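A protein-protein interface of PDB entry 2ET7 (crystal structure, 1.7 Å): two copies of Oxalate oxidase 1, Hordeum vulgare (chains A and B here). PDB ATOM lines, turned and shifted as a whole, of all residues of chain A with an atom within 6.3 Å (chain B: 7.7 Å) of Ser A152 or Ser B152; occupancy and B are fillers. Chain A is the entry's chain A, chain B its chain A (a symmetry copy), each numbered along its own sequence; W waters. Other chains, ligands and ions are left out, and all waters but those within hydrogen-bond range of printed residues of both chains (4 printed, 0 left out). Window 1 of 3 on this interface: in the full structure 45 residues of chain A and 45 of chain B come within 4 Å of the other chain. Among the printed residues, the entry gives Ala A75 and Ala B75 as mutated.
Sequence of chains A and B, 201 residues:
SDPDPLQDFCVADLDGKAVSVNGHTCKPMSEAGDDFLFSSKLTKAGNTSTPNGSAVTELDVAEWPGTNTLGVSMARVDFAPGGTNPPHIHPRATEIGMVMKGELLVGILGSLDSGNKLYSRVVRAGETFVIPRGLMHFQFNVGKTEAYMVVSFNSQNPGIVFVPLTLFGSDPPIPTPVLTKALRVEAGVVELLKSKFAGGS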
ATOM      1  N   VAL A  72     -17.135 -15.479  14.183  1.00  0.00           N
ATOM      2  CA  VAL A  72     -15.671 -15.576  14.381  1.00  0.00           C
ATOM      3  C   VAL A  72     -15.177 -17.044  14.290  1.00  0.00           C
ATOM      4  O   VAL A  72     -15.952 -18.002  14.462  1.00  0.00           O
ATOM      5  CB  VAL A  72     -15.227 -15.017  15.762  1.00  0.00           C
ATOM      6  CG1 VAL A  72     -15.383 -13.472  15.837  1.00  0.00           C
ATOM      7  CG2 VAL A  72     -15.990 -15.727  16.886  1.00  0.00           C
ATOM      8  N   SER A  73     -13.897 -17.188  13.978  1.00  0.00           N
ATOM      9  CA  SER A  73     -13.201 -18.494  14.025  1.00  0.00           C
ATOM     10  C   SER A  73     -11.706 -18.232  14.104  1.00  0.00           C
ATOM     11  O   SER A  73     -11.260 -17.074  13.982  1.00  0.00           O
ATOM     12  CB  SER A  73     -13.521 -19.359  12.800  1.00  0.00           C
ATOM     13  OG  SER A  73     -13.080 -18.774  11.587  1.00  0.00           O
ATOM     14  N   MET A  74     -10.940 -19.312  14.280  1.00  0.00           N
ATOM     15  CA  MET A  74      -9.485 -19.210  14.355  1.00  0.00           C
ATOM     16  C   MET A  74      -8.788 -20.312  13.579  1.00  0.00           C
ATOM     17  O   MET A  74      -9.407 -21.277  13.135  1.00  0.00           O
ATOM     18  CB  MET A  74      -9.035 -19.255  15.821  1.00  0.00           C
ATOM     19  CG  MET A  74      -9.287 -17.977  16.575  1.00  0.00           C
ATOM     20  SD  MET A  74      -8.746 -18.080  18.293  1.00  0.00           S
ATOM     21  CE  MET A  74      -6.994 -17.924  18.077  1.00  0.00           C
ATOM     22  N   ALA A  75      -7.476 -20.172  13.425  1.00  0.00           N
ATOM     23  CA  ALA A  75      -6.673 -21.290  12.952  1.00  0.00           C
ATOM     24  C   ALA A  75      -5.235 -21.075  13.403  1.00  0.00           C
ATOM     25  O   ALA A  75      -4.833 -19.960  13.754  1.00  0.00           O
ATOM     26  CB  ALA A  75      -6.758 -21.434  11.415  1.00  0.00           C
ATOM     27  N   THR A  94     -12.551 -11.630   6.318  1.00  0.00           N
ATOM     28  CA  THR A  94     -11.287 -10.958   6.560  1.00  0.00           C
ATOM     29  C   THR A  94     -10.525 -11.775   7.595  1.00  0.00           C
ATOM     30  O   THR A  94     -11.132 -12.351   8.490  1.00  0.00           O
ATOM     31  CB  THR A  94     -11.566  -9.533   7.062  1.00  0.00           C
ATOM     32  OG1 THR A  94     -12.141  -8.789   5.988  1.00  0.00           O
ATOM     33  CG2 THR A  94     -10.282  -8.816   7.515  1.00  0.00           C
ATOM     34  N   GLU A  95      -9.208 -11.836   7.437  1.00  0.00           N
ATOM     35  CA  GLU A  95      -8.329 -12.536   8.369  1.00  0.00           C
ATOM     36  C   GLU A  95      -7.421 -11.534   9.105  1.00  0.00           C
ATOM     37  O   GLU A  95      -6.926 -10.562   8.509  1.00  0.00           O
ATOM     38  CB  GLU A  95      -7.469 -13.519   7.574  1.00  0.00           C
ATOM     39  CG  GLU A  95      -6.452 -14.267   8.404  1.00  0.00           C
ATOM     40  CD  GLU A  95      -5.612 -15.197   7.564  1.00  0.00           C
ATOM     41  OE1 GLU A  95      -5.929 -15.407   6.364  1.00  0.00           O
ATOM     42  OE2 GLU A  95      -4.612 -15.702   8.109  1.00  0.00           O
ATOM     43  N   ILE A  96      -7.159 -11.801  10.381  1.00  0.00           N
ATOM     44  CA  ILE A  96      -6.235 -10.962  11.158  1.00  0.00           C
ATOM     45  C   ILE A  96      -5.359 -11.909  11.975  1.00  0.00           C
ATOM     46  O   ILE A  96      -5.852 -12.868  12.569  1.00  0.00           O
ATOM     47  CB  ILE A  96      -7.018  -9.892  11.996  1.00  0.00           C
ATOM     48  CG1 ILE A  96      -6.081  -8.796  12.509  1.00  0.00           C
ATOM     49  CG2 ILE A  96      -7.846 -10.541  13.140  1.00  0.00           C
ATOM     50  CD1 ILE A  96      -6.826  -7.530  12.898  1.00  0.00           C
ATOM     51  N   GLY A  97      -4.053 -11.687  11.991  1.00  0.00           N
ATOM     52  CA  GLY A  97      -3.228 -12.710  12.618  1.00  0.00           C
ATOM     53  C   GLY A  97      -1.913 -12.209  13.147  1.00  0.00           C
ATOM     54  O   GLY A  97      -1.541 -11.069  12.914  1.00  0.00           O
ATOM     55  N   VAL A 150      -0.904 -17.598  14.557  1.00  0.00           N
ATOM     56  CA  VAL A 150      -2.271 -17.852  14.986  1.00  0.00           C
ATOM     57  C   VAL A 150      -3.121 -16.764  14.341  1.00  0.00           C
ATOM     58  O   VAL A 150      -2.778 -15.562  14.410  1.00  0.00           O
ATOM     59  CB  VAL A 150      -2.395 -17.832  16.535  1.00  0.00           C
ATOM     60  CG1 VAL A 150      -3.872 -17.853  16.973  1.00  0.00           C
ATOM     61  CG2 VAL A 150      -1.631 -19.015  17.149  1.00  0.00           C
ATOM     62  N   VAL A 151      -4.200 -17.181  13.679  1.00  0.00           N
ATOM     63  CA  VAL A 151      -5.025 -16.227  12.934  1.00  0.00           C
ATOM     64  C   VAL A 151      -6.497 -16.336  13.332  1.00  0.00           C
ATOM     65  O   VAL A 151      -6.945 -17.368  13.847  1.00  0.00           O
ATOM     66  CB  VAL A 151      -4.869 -16.389  11.406  1.00  0.00           C
ATOM     67  CG1 VAL A 151      -3.410 -16.177  10.999  1.00  0.00           C
ATOM     68  CG2 VAL A 151      -5.360 -17.756  10.947  1.00  0.00           C
ATOM     69  N   SER A 152      -7.222 -15.247  13.126  1.00  0.00           N
ATOM     70  CA  SER A 152      -8.643 -15.209  13.423  1.00  0.00           C
ATOM     71  C   SER A 152      -9.379 -14.637  12.225  1.00  0.00           C
ATOM     72  O   SER A 152      -8.767 -13.974  11.379  1.00  0.00           O
ATOM     73  CB  SER A 152      -8.887 -14.345  14.655  1.00  0.00           C
ATOM     74  OG  SER A 152      -8.133 -14.834  15.765  1.00  0.00           O
ATOM     75  N   PHE A 153     -10.678 -14.917  12.134  1.00  0.00           N
ATOM     76  CA  PHE A 153     -11.454 -14.486  10.984  1.00  0.00           C
ATOM     77  C   PHE A 153     -12.785 -13.927  11.464  1.00  0.00           C
ATOM     78  O   PHE A 153     -13.277 -14.346  12.516  1.00  0.00           O
ATOM     79  CB  PHE A 153     -11.756 -15.692  10.085  1.00  0.00           C
ATOM     80  CG  PHE A 153     -10.545 -16.430   9.616  1.00  0.00           C
ATOM     81  CD1 PHE A 153      -9.989 -17.465  10.390  1.00  0.00           C
ATOM     82  CD2 PHE A 153      -9.977 -16.119   8.380  1.00  0.00           C
ATOM     83  CE1 PHE A 153      -8.880 -18.167   9.925  1.00  0.00           C
ATOM     84  CE2 PHE A 153      -8.864 -16.799   7.907  1.00  0.00           C
ATOM     85  CZ  PHE A 153      -8.301 -17.829   8.696  1.00  0.00           C
ATOM     86  N   ASN A 154     -13.393 -13.032  10.679  1.00  0.00           N
ATOM     87  CA  ASN A 154     -14.751 -12.585  11.018  1.00  0.00           C
ATOM     88  C   ASN A 154     -15.840 -13.430  10.345  1.00  0.00           C
ATOM     89  O   ASN A 154     -16.880 -12.913   9.902  1.00  0.00           O
ATOM     90  CB  ASN A 154     -14.927 -11.084  10.777  1.00  0.00           C
ATOM     91  CG  ASN A 154     -14.826 -10.712   9.314  1.00  0.00           C
ATOM     92  OD1 ASN A 154     -14.420 -11.514   8.469  1.00  0.00           O
ATOM     93  ND2 ASN A 154     -15.169  -9.463   9.012  1.00  0.00           N
ATOM     94  N   LEU B  42       1.815  -4.866  19.102  1.00  0.00           N
ATOM     95  CA  LEU B  42       1.574  -5.867  20.154  1.00  0.00           C
ATOM     96  C   LEU B  42       2.810  -6.686  20.534  1.00  0.00           C
ATOM     97  O   LEU B  42       2.696  -7.701  21.226  1.00  0.00           O
ATOM     98  CB  LEU B  42       0.417  -6.797  19.758  1.00  0.00           C
ATOM     99  CG  LEU B  42      -0.907  -6.085  19.455  1.00  0.00           C
ATOM    100  CD1 LEU B  42      -1.993  -7.121  19.195  1.00  0.00           C
ATOM    101  CD2 LEU B  42      -1.344  -5.139  20.585  1.00  0.00           C
ATOM    102  N   VAL B  72     -12.460  -6.227  11.445  1.00  0.00           N
ATOM    103  CA  VAL B  72     -11.613  -6.951  12.418  1.00  0.00           C
ATOM    104  C   VAL B  72     -10.704  -5.982  13.220  1.00  0.00           C
ATOM    105  O   VAL B  72     -10.432  -4.845  12.793  1.00  0.00           O
ATOM    106  CB  VAL B  72     -10.690  -7.996  11.730  1.00  0.00           C
ATOM    107  CG1 VAL B  72     -11.497  -9.198  11.166  1.00  0.00           C
ATOM    108  CG2 VAL B  72      -9.841  -7.316  10.649  1.00  0.00           C
ATOM    109  N   SER B  73     -10.288  -6.440  14.392  1.00  0.00           N
ATOM    110  CA  SER B  73      -9.272  -5.742  15.212  1.00  0.00           C
ATOM    111  C   SER B  73      -8.682  -6.745  16.190  1.00  0.00           C
ATOM    112  O   SER B  73      -9.167  -7.889  16.292  1.00  0.00           O
ATOM    113  CB  SER B  73      -9.868  -4.552  15.972  1.00  0.00           C
ATOM    114  OG  SER B  73     -10.861  -4.941  16.906  1.00  0.00           O
ATOM    115  N   MET B  74      -7.657  -6.301  16.922  1.00  0.00           N
ATOM    116  CA  MET B  74      -7.005  -7.152  17.914  1.00  0.00           C
ATOM    117  C   MET B  74      -6.697  -6.407  19.200  1.00  0.00           C
ATOM    118  O   MET B  74      -6.802  -5.184  19.277  1.00  0.00           O
ATOM    119  CB  MET B  74      -5.706  -7.728  17.334  1.00  0.00           C
ATOM    120  CG  MET B  74      -5.923  -8.840  16.343  1.00  0.00           C
ATOM    121  SD  MET B  74      -4.370  -9.481  15.686  1.00  0.00           S
ATOM    122  CE  MET B  74      -3.826 -10.452  17.066  1.00  0.00           C
ATOM    123  N   ALA B  75      -6.296  -7.155  20.222  1.00  0.00           N
ATOM    124  CA  ALA B  75      -5.710  -6.531  21.398  1.00  0.00           C
ATOM    125  C   ALA B  75      -4.848  -7.563  22.112  1.00  0.00           C
ATOM    126  O   ALA B  75      -4.985  -8.772  21.896  1.00  0.00           O
ATOM    127  CB  ALA B  75      -6.800  -5.969  22.340  1.00  0.00           C
ATOM    128  N   ARG B  76      -3.932  -7.055  22.925  1.00  0.00           N
ATOM    129  CA  ARG B  76      -3.174  -7.881  23.864  1.00  0.00           C
ATOM    130  C   ARG B  76      -3.548  -7.451  25.281  1.00  0.00           C
ATOM    131  O   ARG B  76      -3.745  -6.259  25.548  1.00  0.00           O
ATOM    132  CB  ARG B  76      -1.689  -7.687  23.595  1.00  0.00           C
ATOM    133  CG  ARG B  76      -0.773  -8.241  24.643  1.00  0.00           C
ATOM    134  CD  ARG B  76       0.708  -8.113  24.245  1.00  0.00           C
ATOM    135  NE  ARG B  76       1.530  -8.586  25.363  1.00  0.00           N
ATOM    136  CZ  ARG B  76       2.702  -9.205  25.244  1.00  0.00           C
ATOM    137  NH1 ARG B  76       3.244  -9.417  24.047  1.00  0.00           N
ATOM    138  NH2 ARG B  76       3.344  -9.605  26.337  1.00  0.00           N
ATOM    139  N   HIS B  90     -18.081  -5.829  25.294  1.00  0.00           N
ATOM    140  CA  HIS B  90     -17.761  -5.160  24.024  1.00  0.00           C
ATOM    141  C   HIS B  90     -19.084  -4.969  23.318  1.00  0.00           C
ATOM    142  O   HIS B  90     -19.702  -5.951  22.916  1.00  0.00           O
ATOM    143  CB  HIS B  90     -16.821  -6.012  23.169  1.00  0.00           C
ATOM    144  CG  HIS B  90     -15.567  -6.355  23.881  1.00  0.00           C
ATOM    145  ND1 HIS B  90     -14.658  -5.389  24.251  1.00  0.00           N
ATOM    146  CD2 HIS B  90     -15.112  -7.527  24.388  1.00  0.00           C
ATOM    147  CE1 HIS B  90     -13.665  -5.958  24.918  1.00  0.00           C
ATOM    148  NE2 HIS B  90     -13.921  -7.249  25.022  1.00  0.00           N
ATOM    149  N   ALA B  93     -18.974  -6.198  19.153  1.00  0.00           N
ATOM    150  CA  ALA B  93     -18.206  -7.309  18.546  1.00  0.00           C
ATOM    151  C   ALA B  93     -18.199  -8.534  19.416  1.00  0.00           C
ATOM    152  O   ALA B  93     -18.190  -8.431  20.649  1.00  0.00           O
ATOM    153  CB  ALA B  93     -16.753  -6.887  18.315  1.00  0.00           C
ATOM    154  N   THR B  94     -18.157  -9.681  18.747  1.00  0.00           N
ATOM    155  CA  THR B  94     -17.761 -10.942  19.346  1.00  0.00           C
ATOM    156  C   THR B  94     -16.242 -10.935  19.466  1.00  0.00           C
ATOM    157  O   THR B  94     -15.562 -10.386  18.608  1.00  0.00           O
ATOM    158  CB  THR B  94     -18.249 -12.095  18.455  1.00  0.00           C
ATOM    159  OG1 THR B  94     -19.675 -12.128  18.515  1.00  0.00           O
ATOM    160  CG2 THR B  94     -17.713 -13.458  18.924  1.00  0.00           C
ATOM    161  N   GLU B  95     -15.739 -11.521  20.546  1.00  0.00           N
ATOM    162  CA  GLU B  95     -14.305 -11.643  20.786  1.00  0.00           C
ATOM    163  C   GLU B  95     -13.875 -13.120  20.728  1.00  0.00           C
ATOM    164  O   GLU B  95     -14.590 -14.013  21.213  1.00  0.00           O
ATOM    165  CB  GLU B  95     -13.998 -11.074  22.172  1.00  0.00           C
ATOM    166  CG  GLU B  95     -12.552 -11.201  22.591  1.00  0.00           C
ATOM    167  CD  GLU B  95     -12.315 -10.654  23.977  1.00  0.00           C
ATOM    168  OE1 GLU B  95     -13.229 -10.007  24.553  1.00  0.00           O
ATOM    169  OE2 GLU B  95     -11.210 -10.897  24.498  1.00  0.00           O
ATOM    170  N   ILE B  96     -12.686 -13.369  20.188  1.00  0.00           N
ATOM    171  CA  ILE B  96     -12.135 -14.732  20.158  1.00  0.00           C
ATOM    172  C   ILE B  96     -10.659 -14.620  20.533  1.00  0.00           C
ATOM    173  O   ILE B  96      -9.951 -13.738  20.049  1.00  0.00           O
ATOM    174  CB  ILE B  96     -12.420 -15.422  18.779  1.00  0.00           C
ATOM    175  CG1 ILE B  96     -12.190 -16.933  18.858  1.00  0.00           C
ATOM    176  CG2 ILE B  96     -11.618 -14.764  17.622  1.00  0.00           C
ATOM    177  CD1 ILE B  96     -12.887 -17.687  17.738  1.00  0.00           C
ATOM    178  N   GLY B  97     -10.179 -15.477  21.422  1.00  0.00           N
ATOM    179  CA  GLY B  97      -8.825 -15.228  21.899  1.00  0.00           C
ATOM    180  C   GLY B  97      -8.109 -16.451  22.399  1.00  0.00           C
ATOM    181  O   GLY B  97      -8.699 -17.514  22.522  1.00  0.00           O
ATOM    182  N   MET B  98      -6.824 -16.278  22.669  1.00  0.00           N
ATOM    183  CA  MET B  98      -5.979 -17.385  23.075  1.00  0.00           C
ATOM    184  C   MET B  98      -5.082 -16.905  24.199  1.00  0.00           C
ATOM    185  O   MET B  98      -4.524 -15.804  24.114  1.00  0.00           O
ATOM    186  CB  MET B  98      -5.124 -17.833  21.887  1.00  0.00           C
ATOM    187  CG  MET B  98      -4.233 -19.022  22.170  1.00  0.00           C
ATOM    188  SD  MET B  98      -3.123 -19.335  20.778  1.00  0.00           S
ATOM    189  CE  MET B  98      -4.113 -20.454  19.823  1.00  0.00           C
ATOM    190  N   PHE B 129     -10.927 -19.185  23.787  1.00  0.00           N
ATOM    191  CA  PHE B 129     -12.264 -18.900  24.291  1.00  0.00           C
ATOM    192  C   PHE B 129     -12.945 -17.954  23.307  1.00  0.00           C
ATOM    193  O   PHE B 129     -12.281 -17.250  22.520  1.00  0.00           O
ATOM    194  CB  PHE B 129     -12.191 -18.266  25.694  1.00  0.00           C
ATOM    195  CG  PHE B 129     -11.326 -17.024  25.760  1.00  0.00           C
ATOM    196  CD1 PHE B 129     -11.870 -15.757  25.482  1.00  0.00           C
ATOM    197  CD2 PHE B 129      -9.976 -17.118  26.116  1.00  0.00           C
ATOM    198  CE1 PHE B 129     -11.064 -14.617  25.532  1.00  0.00           C
ATOM    199  CE2 PHE B 129      -9.163 -15.967  26.180  1.00  0.00           C
ATOM    200  CZ  PHE B 129      -9.725 -14.715  25.877  1.00  0.00           C
ATOM    201  N   VAL B 130     -14.271 -17.943  23.359  1.00  0.00           N
ATOM    202  CA  VAL B 130     -15.072 -17.065  22.502  1.00  0.00           C
ATOM    203  C   VAL B 130     -16.162 -16.399  23.343  1.00  0.00           C
ATOM    204  O   VAL B 130     -16.793 -17.049  24.184  1.00  0.00           O
ATOM    205  CB  VAL B 130     -15.615 -17.805  21.235  1.00  0.00           C
ATOM    206  CG1 VAL B 130     -16.619 -18.898  21.606  1.00  0.00           C
ATOM    207  CG2 VAL B 130     -16.242 -16.794  20.256  1.00  0.00           C
ATOM    208  N   ILE B 131     -16.351 -15.093  23.126  1.00  0.00           N
ATOM    209  CA  ILE B 131     -17.272 -14.288  23.928  1.00  0.00           C
ATOM    210  C   ILE B 131     -18.236 -13.573  22.997  1.00  0.00           C
ATOM    211  O   ILE B 131     -17.824 -12.678  22.266  1.00  0.00           O
ATOM    212  CB  ILE B 131     -16.534 -13.188  24.738  1.00  0.00           C
ATOM    213  CG1 ILE B 131     -15.272 -13.732  25.432  1.00  0.00           C
ATOM    214  CG2 ILE B 131     -17.521 -12.451  25.645  1.00  0.00           C
ATOM    215  CD1 ILE B 131     -15.488 -14.360  26.697  1.00  0.00           C
ATOM    216  N   VAL B 150      -3.856 -12.931  23.656  1.00  0.00           N
ATOM    217  CA  VAL B 150      -4.021 -12.132  22.450  1.00  0.00           C
ATOM    218  C   VAL B 150      -5.432 -12.418  21.950  1.00  0.00           C
ATOM    219  O   VAL B 150      -5.846 -13.594  21.845  1.00  0.00           O
ATOM    220  CB  VAL B 150      -2.952 -12.488  21.381  1.00  0.00           C
ATOM    221  CG1 VAL B 150      -3.279 -11.826  20.028  1.00  0.00           C
ATOM    222  CG2 VAL B 150      -1.553 -12.074  21.863  1.00  0.00           C
ATOM    223  N   VAL B 151      -6.185 -11.349  21.684  1.00  0.00           N
ATOM    224  CA  VAL B 151      -7.589 -11.512  21.299  1.00  0.00           C
ATOM    225  C   VAL B 151      -7.898 -10.770  19.999  1.00  0.00           C
ATOM    226  O   VAL B 151      -7.191  -9.830  19.615  1.00  0.00           O
ATOM    227  CB  VAL B 151      -8.556 -11.062  22.416  1.00  0.00           C
ATOM    228  CG1 VAL B 151      -8.312 -11.879  23.686  1.00  0.00           C
ATOM    229  CG2 VAL B 151      -8.409  -9.572  22.701  1.00  0.00           C
ATOM    230  N   SER B 152      -8.931 -11.234  19.314  1.00  0.00           N
ATOM    231  CA  SER B 152      -9.367 -10.613  18.075  1.00  0.00           C
ATOM    232  C   SER B 152     -10.867 -10.390  18.140  1.00  0.00           C
ATOM    233  O   SER B 152     -11.556 -11.026  18.948  1.00  0.00           O
ATOM    234  CB  SER B 152      -9.017 -11.514  16.897  1.00  0.00           C
ATOM    235  OG  SER B 152      -7.617 -11.791  16.879  1.00  0.00           O
ATOM    236  N   PHE B 153     -11.370  -9.471  17.318  1.00  0.00           N
ATOM    237  CA  PHE B 153     -12.781  -9.124  17.361  1.00  0.00           C
ATOM    238  C   PHE B 153     -13.310  -9.022  15.937  1.00  0.00           C
ATOM    239  O   PHE B 153     -12.543  -8.701  15.025  1.00  0.00           O
ATOM    240  CB  PHE B 153     -12.955  -7.749  18.018  1.00  0.00           C
ATOM    241  CG  PHE B 153     -12.378  -7.646  19.393  1.00  0.00           C
ATOM    242  CD1 PHE B 153     -11.031  -7.287  19.583  1.00  0.00           C
ATOM    243  CD2 PHE B 153     -13.191  -7.870  20.505  1.00  0.00           C
ATOM    244  CE1 PHE B 153     -10.517  -7.162  20.871  1.00  0.00           C
ATOM    245  CE2 PHE B 153     -12.692  -7.763  21.795  1.00  0.00           C
ATOM    246  CZ  PHE B 153     -11.333  -7.416  21.980  1.00  0.00           C
ATOM    247  N   ASN B 154     -14.615  -9.237  15.753  1.00  0.00           N
ATOM    248  CA  ASN B 154     -15.203  -8.994  14.428  1.00  0.00           C
ATOM    249  C   ASN B 154     -15.748  -7.568  14.272  1.00  0.00           C
ATOM    250  O   ASN B 154     -16.802  -7.341  13.655  1.00  0.00           O
ATOM    251  CB  ASN B 154     -16.229 -10.067  14.060  1.00  0.00           C
ATOM    252  CG  ASN B 154     -17.448 -10.042  14.957  1.00  0.00           C
ATOM    253  OD1 ASN B 154     -17.474  -9.375  15.994  1.00  0.00           O
ATOM    254  ND2 ASN B 154     -18.464 -10.808  14.570  1.00  0.00           N
ATOM    255  N   SER B 155     -15.000  -6.609  14.830  1.00  0.00           N
ATOM    256  CA  SER B 155     -15.220  -5.195  14.565  1.00  0.00           C
ATOM    257  C   SER B 155     -13.882  -4.472  14.549  1.00  0.00           C
ATOM    258  O   SER B 155     -12.928  -4.867  15.252  1.00  0.00           O
ATOM    259  CB  SER B 155     -16.122  -4.543  15.627  1.00  0.00           C
ATOM    260  OG  SER B 155     -16.295  -3.147  15.363  1.00  0.00           O
ATOM    261  N   PRO B 158     -14.529  -2.468  18.616  1.00  0.00           N
ATOM    262  CA  PRO B 158     -15.497  -3.208  19.424  1.00  0.00           C
ATOM    263  C   PRO B 158     -16.068  -2.402  20.577  1.00  0.00           C
ATOM    264  O   PRO B 158     -17.217  -2.627  20.943  1.00  0.00           O
ATOM    265  CB  PRO B 158     -14.718  -4.418  19.942  1.00  0.00           C
ATOM    266  CG  PRO B 158     -13.320  -4.221  19.585  1.00  0.00           C
ATOM    267  CD  PRO B 158     -13.172  -3.044  18.650  1.00  0.00           C
HETATM  268  O   HOH W   1      -5.879 -13.227  15.455  1.00  0.00           O
HETATM  269  O   HOH W   2     -18.523 -11.085  11.483  1.00  0.00           O
HETATM  270  O   HOH W   3      -7.664 -14.182  18.308  1.00  0.00           O
HETATM  271  O   HOH W   4     -17.316  -8.402  10.982  1.00  0.00           O
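Val A72 touches Thr B94, and with the chains exchanged Thr A94 touches Val B72.
Ser A73 touches Ile B96, and with the chains exchanged Ile A96 touches Ser B73.
Ile A96 touches Ser B152, and with the chains exchanged Ser A152 touches Ile B96.
Asn A154 touches its own counterpart, Asn B154.
Positions printed for both chains: 72, 73, 74, 75, 94, 95, 96, 97, 150, 151, 152, 153 and 154.
Of the 16 pairs that touch across the chains among the printed residues, 14 have their exchanged pair printed and touching as well.
OG of Ser B152 is in hydrogen-bond range of OG of Ser A152 (3.3 Å).
The side-chain amide oxygen (OD1) of Asn A154 is in hydrogen-bond range of the backbone NH (N) of Thr A94 (2.9 Å).
N of Ser A152 lies within hydrogen-bond range of O of Ile A96 (2.8 Å).
N of Phe B153 sits at hydrogen-bond distance from O of Ser B73, at 2.9 Å.
The side-chain hydroxyl of Ser B73 sits at hydrogen-bond distance from the backbone carbonyl oxygen of Ser B155, 2.6 Å away.
O of Ile B96 is in hydrogen-bond range of N of Ser B152, at 2.8 Å.
The backbone NH (N) of Met B98 sits at hydrogen-bond distance from the backbone carbonyl oxygen (O) of Val B150 (3.0 Å).
Val A72 touches Ile B96.
Met A74 touches Ile B96.
CG2 of Thr A94 touches CG2 of Val B72 (3.5 Å).
Ile A96 touches Val B72 (CD1 to CG2, 3.8 Å).
CD1 of Ile A96 touches CA of Ser B73, at 3.8 Å.
SD of Met B74 touches CG1 of Ile A96 (3.7 Å).
CG2 of Ile A96 touches OG of Ser B152, at 3.9 Å.
CG1 of Val A150 touches CE of Met B98 (3.9 Å).
Val B72 touches Asn A154 (CG1 to CB, 3.9 Å).
Asn A154 touches Asn B154.
Of the printed residues of chain B, Ser A152 touches Ile B96 (3.9 Å) and Ser B152 (3.3 Å).
Of chain A, only Ile A96 and Ser A152 come within 4 Å of Ser B152.
Of the printed residues of chain A, Met B74 touches Ile A96 (3.7 Å).
Printed residues of chain A within 4 Å of Val B72: Thr A94 (3.5 Å), Ile A96 (3.8 Å) and Asn A154 (3.9 Å).
Of the printed residues of chain A, Val B130 touches Val A72.
Of the printed residues of chain B, Met A74 touches Ile B96.
Leu B42 touches none of the printed residues of chain A.
Ala B93 touches none of the printed residues of chain A.
The nearest residue of chain B that does not touch Ser A152 is Val B72 (5.5 Å).
The nearest printed residue of chain A that does not touch Met B74 is Gly A97 (4.3 Å).
Water W3 lies within hydrogen-bond range of OG of Ser A152, OG of Ser B152 and O of Ile B96.
Water W1 lies within hydrogen-bond range of OG of Ser B152 (2.7 Å), OG of Ser A152 (2.8 Å) and O of Ile A96 (2.9 Å).
Water W2 bridges O of Asn A154 and ND2 of Asn B154.
Water W4 lies within hydrogen-bond range of the backbone carbonyl oxygen (O) of Asn B154 (2.9 Å) and the side-chain amide nitrogen (ND2) of Asn A154 (3.1 Å).
Printed residues of chain A that touch a printed residue of chain B: Val A72, Ser A73, Met A74, Thr A94, Ile A96, Val A150, Ser A152 and Asn A154.
Hydrophobic or aromatic side chains of chain A that line the printed part of chain B: Val A72, Met A74, Ile A96 and Val A150.
Among the printed residues, no Asp or Glu carboxylate lies within 4 Å of a Lys or Arg side-chain nitrogen of the other chain.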
